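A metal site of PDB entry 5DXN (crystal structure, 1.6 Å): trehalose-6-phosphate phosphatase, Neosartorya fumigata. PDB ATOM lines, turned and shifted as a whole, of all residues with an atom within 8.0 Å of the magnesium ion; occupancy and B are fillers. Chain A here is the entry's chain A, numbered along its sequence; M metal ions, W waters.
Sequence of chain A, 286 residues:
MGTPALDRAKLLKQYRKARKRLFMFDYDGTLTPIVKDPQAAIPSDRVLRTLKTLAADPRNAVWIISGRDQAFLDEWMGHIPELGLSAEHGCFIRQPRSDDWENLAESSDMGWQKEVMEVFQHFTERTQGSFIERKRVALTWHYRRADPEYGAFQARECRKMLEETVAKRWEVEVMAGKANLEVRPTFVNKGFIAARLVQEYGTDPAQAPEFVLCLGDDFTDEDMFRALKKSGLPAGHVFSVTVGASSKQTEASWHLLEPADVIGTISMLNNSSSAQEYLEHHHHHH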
ATOM      1  N   PHE A  25      21.319 -15.271  -2.578  1.00  0.00           N
ATOM      2  CA  PHE A  25      20.865 -15.210  -1.201  1.00  0.00           C
ATOM      3  C   PHE A  25      21.881 -15.843  -0.270  1.00  0.00           C
ATOM      4  O   PHE A  25      22.163 -17.026  -0.425  1.00  0.00           O
ATOM      5  CB  PHE A  25      19.557 -15.967  -0.986  1.00  0.00           C
ATOM      6  CG  PHE A  25      18.389 -15.464  -1.775  1.00  0.00           C
ATOM      7  CD1 PHE A  25      18.167 -14.114  -1.938  1.00  0.00           C
ATOM      8  CD2 PHE A  25      17.493 -16.342  -2.322  1.00  0.00           C
ATOM      9  CE1 PHE A  25      17.048 -13.665  -2.667  1.00  0.00           C
ATOM     10  CE2 PHE A  25      16.379 -15.902  -3.031  1.00  0.00           C
ATOM     11  CZ  PHE A  25      16.165 -14.571  -3.194  1.00  0.00           C
ATOM     12  N   ASP A  26      22.378 -15.088   0.694  1.00  0.00           N
ATOM     13  CA  ASP A  26      22.978 -15.700   1.878  1.00  0.00           C
ATOM     14  C   ASP A  26      21.894 -16.493   2.612  1.00  0.00           C
ATOM     15  O   ASP A  26      20.711 -16.156   2.490  1.00  0.00           O
ATOM     16  CB  ASP A  26      23.588 -14.627   2.797  1.00  0.00           C
ATOM     17  CG  ASP A  26      24.087 -15.184   4.116  1.00  0.00           C
ATOM     18  OD1 ASP A  26      24.860 -16.149   4.067  1.00  0.00           O
ATOM     19  OD2 ASP A  26      23.681 -14.669   5.178  1.00  0.00           O
ATOM     20  N   TYR A  27      22.266 -17.539   3.360  1.00  0.00           N
ATOM     21  CA  TYR A  27      21.290 -18.296   4.127  1.00  0.00           C
ATOM     22  C   TYR A  27      21.132 -17.795   5.555  1.00  0.00           C
ATOM     23  O   TYR A  27      20.157 -17.132   5.884  1.00  0.00           O
ATOM     24  CB  TYR A  27      21.657 -19.780   4.155  1.00  0.00           C
ATOM     25  CG  TYR A  27      20.623 -20.562   4.895  1.00  0.00           C
ATOM     26  CD1 TYR A  27      19.342 -20.702   4.381  1.00  0.00           C
ATOM     27  CD2 TYR A  27      20.909 -21.144   6.127  1.00  0.00           C
ATOM     28  CE1 TYR A  27      18.364 -21.417   5.066  1.00  0.00           C
ATOM     29  CE2 TYR A  27      19.943 -21.865   6.812  1.00  0.00           C
ATOM     30  CZ  TYR A  27      18.680 -21.997   6.286  1.00  0.00           C
ATOM     31  OH  TYR A  27      17.734 -22.710   6.970  1.00  0.00           O
ATOM     32  N   ASP A  28      22.104 -18.078   6.419  1.00  0.00           N
ATOM     33  CA  ASP A  28      21.956 -17.757   7.832  1.00  0.00           C
ATOM     34  C   ASP A  28      21.866 -16.264   8.108  1.00  0.00           C
ATOM     35  O   ASP A  28      22.742 -15.494   7.688  1.00  0.00           O
ATOM     36  CB  ASP A  28      23.119 -18.350   8.623  1.00  0.00           C
ATOM     37  CG  ASP A  28      22.972 -19.855   8.811  1.00  0.00           C
ATOM     38  OD1 ASP A  28      22.053 -20.263   9.555  1.00  0.00           O
ATOM     39  OD2 ASP A  28      23.765 -20.618   8.215  1.00  0.00           O
ATOM     40  N   GLY A  29      20.825 -15.866   8.848  1.00  0.00           N
ATOM     41  CA  GLY A  29      20.616 -14.466   9.194  1.00  0.00           C
ATOM     42  C   GLY A  29      19.902 -13.695   8.112  1.00  0.00           C
ATOM     43  O   GLY A  29      19.526 -12.540   8.304  1.00  0.00           O
ATOM     44  N   THR A  30      19.676 -14.347   6.980  1.00  0.00           N
ATOM     45  CA  THR A  30      19.103 -13.691   5.813  1.00  0.00           C
ATOM     46  C   THR A  30      17.773 -14.340   5.415  1.00  0.00           C
ATOM     47  O   THR A  30      16.732 -13.672   5.447  1.00  0.00           O
ATOM     48  CB  THR A  30      20.096 -13.708   4.645  1.00  0.00           C
ATOM     49  OG1 THR A  30      21.281 -13.001   5.030  1.00  0.00           O
ATOM     50  CG2 THR A  30      19.492 -13.098   3.391  1.00  0.00           C
ATOM     51  N   LEU A  31      17.817 -15.613   5.045  1.00  0.00           N
ATOM     52  CA  LEU A  31      16.594 -16.369   4.764  1.00  0.00           C
ATOM     53  C   LEU A  31      15.964 -16.936   6.047  1.00  0.00           C
ATOM     54  O   LEU A  31      14.781 -17.250   6.062  1.00  0.00           O
ATOM     55  CB  LEU A  31      16.870 -17.492   3.766  1.00  0.00           C
ATOM     56  CG  LEU A  31      17.104 -17.071   2.308  1.00  0.00           C
ATOM     57  CD1 LEU A  31      17.625 -18.232   1.488  1.00  0.00           C
ATOM     58  CD2 LEU A  31      15.840 -16.499   1.654  1.00  0.00           C
ATOM     59  N   THR A  32      16.756 -17.044   7.107  1.00  0.00           N
ATOM     60  CA  THR A  32      16.282 -17.599   8.381  1.00  0.00           C
ATOM     61  C   THR A  32      16.981 -16.879   9.535  1.00  0.00           C
ATOM     62  O   THR A  32      18.090 -16.390   9.358  1.00  0.00           O
ATOM     63  CB  THR A  32      16.542 -19.129   8.466  1.00  0.00           C
ATOM     64  OG1 THR A  32      15.746 -19.701   9.519  1.00  0.00           O
ATOM     65  CG2 THR A  32      18.024 -19.436   8.691  1.00  0.00           C
ATOM     66  N   ILE A  34      19.232 -16.063  12.832  1.00  0.00           N
ATOM     67  CA  ILE A  34      20.387 -16.659  13.483  1.00  0.00           C
ATOM     68  C   ILE A  34      19.934 -17.336  14.779  1.00  0.00           C
ATOM     69  O   ILE A  34      19.107 -16.804  15.514  1.00  0.00           O
ATOM     70  CB  ILE A  34      21.492 -15.617  13.814  1.00  0.00           C
ATOM     71  CG1 ILE A  34      21.976 -14.905  12.545  1.00  0.00           C
ATOM     72  CG2 ILE A  34      22.680 -16.286  14.505  1.00  0.00           C
ATOM     73  CD1 ILE A  34      22.833 -15.739  11.667  1.00  0.00           C
ATOM     74  N   ILE A  65      23.863 -19.111  -1.148  1.00  0.00           N
ATOM     75  CA  ILE A  65      25.311 -19.031  -0.942  1.00  0.00           C
ATOM     76  C   ILE A  65      25.599 -19.113   0.536  1.00  0.00           C
ATOM     77  O   ILE A  65      25.288 -18.178   1.291  1.00  0.00           O
ATOM     78  CB  ILE A  65      25.919 -17.756  -1.521  1.00  0.00           C
ATOM     79  CG1 ILE A  65      25.587 -17.595  -3.010  1.00  0.00           C
ATOM     80  CG2 ILE A  65      27.454 -17.781  -1.338  1.00  0.00           C
ATOM     81  CD1 ILE A  65      25.842 -16.197  -3.552  1.00  0.00           C
ATOM     82  N   SER A  66      26.200 -20.215   0.952  1.00  0.00           N
ATOM     83  CA  SER A  66      26.292 -20.542   2.358  1.00  0.00           C
ATOM     84  C   SER A  66      27.637 -21.134   2.788  1.00  0.00           C
ATOM     85  O   SER A  66      28.329 -21.789   2.014  1.00  0.00           O
ATOM     86  CB  SER A  66      25.185 -21.518   2.727  1.00  0.00           C
ATOM     87  OG  SER A  66      25.167 -21.740   4.117  1.00  0.00           O
ATOM     88  N   GLY A  67      27.967 -20.938   4.057  1.00  0.00           N
ATOM     89  CA  GLY A  67      29.105 -21.607   4.641  1.00  0.00           C
ATOM     90  C   GLY A  67      28.695 -22.940   5.220  1.00  0.00           C
ATOM     91  O   GLY A  67      29.550 -23.707   5.673  1.00  0.00           O
ATOM     92  N   LYS A 190      32.854 -14.492  -0.990  1.00  0.00           N
ATOM     93  CA  LYS A 190      31.504 -14.292  -1.529  1.00  0.00           C
ATOM     94  C   LYS A 190      31.464 -13.269  -2.656  1.00  0.00           C
ATOM     95  O   LYS A 190      30.614 -13.359  -3.557  1.00  0.00           O
ATOM     96  CB  LYS A 190      30.525 -13.856  -0.423  1.00  0.00           C
ATOM     97  CG  LYS A 190      29.798 -14.986   0.249  1.00  0.00           C
ATOM     98  CD  LYS A 190      28.645 -14.461   1.103  1.00  0.00           C
ATOM     99  CE  LYS A 190      28.551 -15.214   2.420  1.00  0.00           C
ATOM    100  NZ  LYS A 190      27.308 -14.901   3.194  1.00  0.00           N
ATOM    101  N   LEU A 215      21.268 -10.481  -1.288  1.00  0.00           N
ATOM    102  CA  LEU A 215      20.867 -10.311   0.103  1.00  0.00           C
ATOM    103  C   LEU A 215      21.847 -10.958   1.077  1.00  0.00           C
ATOM    104  O   LEU A 215      22.229 -12.101   0.874  1.00  0.00           O
ATOM    105  CB  LEU A 215      19.475 -10.919   0.339  1.00  0.00           C
ATOM    106  CG  LEU A 215      18.264 -10.140  -0.164  1.00  0.00           C
ATOM    107  CD1 LEU A 215      17.142 -11.070  -0.527  1.00  0.00           C
ATOM    108  CD2 LEU A 215      17.778  -9.246   0.942  1.00  0.00           C
ATOM    109  N   GLY A 216      22.235 -10.239   2.128  1.00  0.00           N
ATOM    110  CA  GLY A 216      23.028 -10.868   3.171  1.00  0.00           C
ATOM    111  C   GLY A 216      23.027 -10.019   4.431  1.00  0.00           C
ATOM    112  O   GLY A 216      22.606  -8.873   4.385  1.00  0.00           O
ATOM    113  N   ASP A 217      23.538 -10.561   5.539  1.00  0.00           N
ATOM    114  CA  ASP A 217      23.345  -9.945   6.836  1.00  0.00           C
ATOM    115  C   ASP A 217      24.623  -9.555   7.585  1.00  0.00           C
ATOM    116  O   ASP A 217      24.549  -8.835   8.562  1.00  0.00           O
ATOM    117  CB  ASP A 217      22.517 -10.878   7.749  1.00  0.00           C
ATOM    118  CG  ASP A 217      23.286 -12.148   8.140  1.00  0.00           C
ATOM    119  OD1 ASP A 217      23.759 -12.873   7.240  1.00  0.00           O
ATOM    120  OD2 ASP A 217      23.438 -12.417   9.351  1.00  0.00           O
ATOM    121  N   ASP A 218      25.793 -10.029   7.140  1.00  0.00           N
ATOM    122  CA  ASP A 218      27.009  -9.720   7.904  1.00  0.00           C
ATOM    123  C   ASP A 218      28.193  -9.288   7.044  1.00  0.00           C
ATOM    124  O   ASP A 218      28.064  -9.073   5.844  1.00  0.00           O
ATOM    125  CB  ASP A 218      27.403 -10.919   8.815  1.00  0.00           C
ATOM    126  CG  ASP A 218      27.974 -12.113   8.053  1.00  0.00           C
ATOM    127  OD1 ASP A 218      28.481 -11.977   6.918  1.00  0.00           O
ATOM    128  OD2 ASP A 218      27.951 -13.228   8.624  1.00  0.00           O
ATOM    129  N   PHE A 219      29.365  -9.161   7.646  1.00  0.00           N
ATOM    130  CA  PHE A 219      30.520  -8.609   6.944  1.00  0.00           C
ATOM    131  C   PHE A 219      30.943  -9.422   5.719  1.00  0.00           C
ATOM    132  O   PHE A 219      31.511  -8.858   4.780  1.00  0.00           O
ATOM    133  CB  PHE A 219      31.710  -8.464   7.905  1.00  0.00           C
ATOM    134  CG  PHE A 219      32.312  -9.772   8.326  1.00  0.00           C
ATOM    135  CD1 PHE A 219      33.463 -10.253   7.712  1.00  0.00           C
ATOM    136  CD2 PHE A 219      31.730 -10.525   9.330  1.00  0.00           C
ATOM    137  CE1 PHE A 219      34.020 -11.461   8.102  1.00  0.00           C
ATOM    138  CE2 PHE A 219      32.282 -11.745   9.722  1.00  0.00           C
ATOM    139  CZ  PHE A 219      33.425 -12.209   9.108  1.00  0.00           C
ATOM    140  N   THR A 220      30.692 -10.732   5.728  1.00  0.00           N
ATOM    141  CA  THR A 220      31.100 -11.572   4.604  1.00  0.00           C
ATOM    142  C   THR A 220      30.288 -11.212   3.369  1.00  0.00           C
ATOM    143  O   THR A 220      30.774 -11.335   2.242  1.00  0.00           O
ATOM    144  CB  THR A 220      30.954 -13.087   4.893  1.00  0.00           C
ATOM    145  OG1 THR A 220      29.567 -13.433   5.061  1.00  0.00           O
ATOM    146  CG2 THR A 220      31.760 -13.483   6.130  1.00  0.00           C
ATOM    147  N   ASP A 221      29.066 -10.729   3.596  1.00  0.00           N
ATOM    148  CA  ASP A 221      28.150 -10.379   2.526  1.00  0.00           C
ATOM    149  C   ASP A 221      28.471  -9.019   1.921  1.00  0.00           C
ATOM    150  O   ASP A 221      28.070  -8.713   0.804  1.00  0.00           O
ATOM    151  CB  ASP A 221      26.704 -10.402   3.030  1.00  0.00           C
ATOM    152  CG  ASP A 221      26.333 -11.752   3.588  1.00  0.00           C
ATOM    153  OD1 ASP A 221      26.424 -12.735   2.827  1.00  0.00           O
ATOM    154  OD2 ASP A 221      26.016 -11.839   4.790  1.00  0.00           O
ATOM    155  N   VAL A 243      20.532  -7.184   5.471  1.00  0.00           N
ATOM    156  CA  VAL A 243      19.540  -7.481   6.477  1.00  0.00           C
ATOM    157  C   VAL A 243      20.057  -6.945   7.806  1.00  0.00           C
ATOM    158  O   VAL A 243      21.042  -7.440   8.344  1.00  0.00           O
ATOM    159  CB  VAL A 243      19.276  -8.981   6.561  1.00  0.00           C
ATOM    160  CG1 VAL A 243      18.240  -9.264   7.630  1.00  0.00           C
ATOM    161  CG2 VAL A 243      18.818  -9.481   5.198  1.00  0.00           C
HETATM  162 MG    MG M   1      24.480 -14.751   6.988  1.00  0.00          MG
HETATM  163  O   HOH W   1      25.358 -16.628   6.817  1.00  0.00           O
HETATM  164  O   HOH W   2      25.050 -14.593   9.006  1.00  0.00           O
HETATM  165  O   HOH W   3      26.217 -13.922   6.336  1.00  0.00           O
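Asp 221 touches the magnesium ion (OD2 to MG, 3.96 Å). The nearest printed residue that does not touch the magnesium ion is Asp 218 (4.1 Å).
The side-chain carboxylate of Asp 26 sits close to the side-chain hydroxyl of Thr 30 (2.9 Å). The side-chain carboxylate (OD1) of Asp 26 lies within salt-bridge range of the side-chain amino group (NZ) of Lys 190. The backbone carbonyl oxygen (O) of Leu 215 is in hydrogen-bond range of the backbone NH (N) of Asp 26. The backbone NH (N) of Asp 217 is in hydrogen-bond range of the side-chain carboxylate (OD2) of Asp 221 (2.9 Å). OG1 of Thr 30 sits at hydrogen-bond distance from N of Asp 217 (3.4 Å). The side-chain carboxylate of Asp 221 is in hydrogen-bond range of the backbone NH of Asp 218. The side-chain carboxylate (OD2) of Asp 221 is in salt-bridge range of the side-chain amino group (NZ) of Lys 190 (3.7 Å).
The magnesium ion is bound by the side-chain carboxylate (OD2) of Asp 26 (2.0 Å). The backbone carbonyl oxygen (O) of Asp 28 binds the magnesium ion (2.0 Å). The magnesium ion is bound by OD1 of Asp 217 (2.0 Å). Water W3 is bound to the magnesium ion (2.0 Å). The magnesium ion is bound by water W1 (2.1 Å). Water W2 is bound to the magnesium ion (2.1 Å). The magnesium ion has six donor atoms within binding distance.
Water W2 lies within hydrogen-bond range of OD2 of Asp 217 and OD2 of Asp 218.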
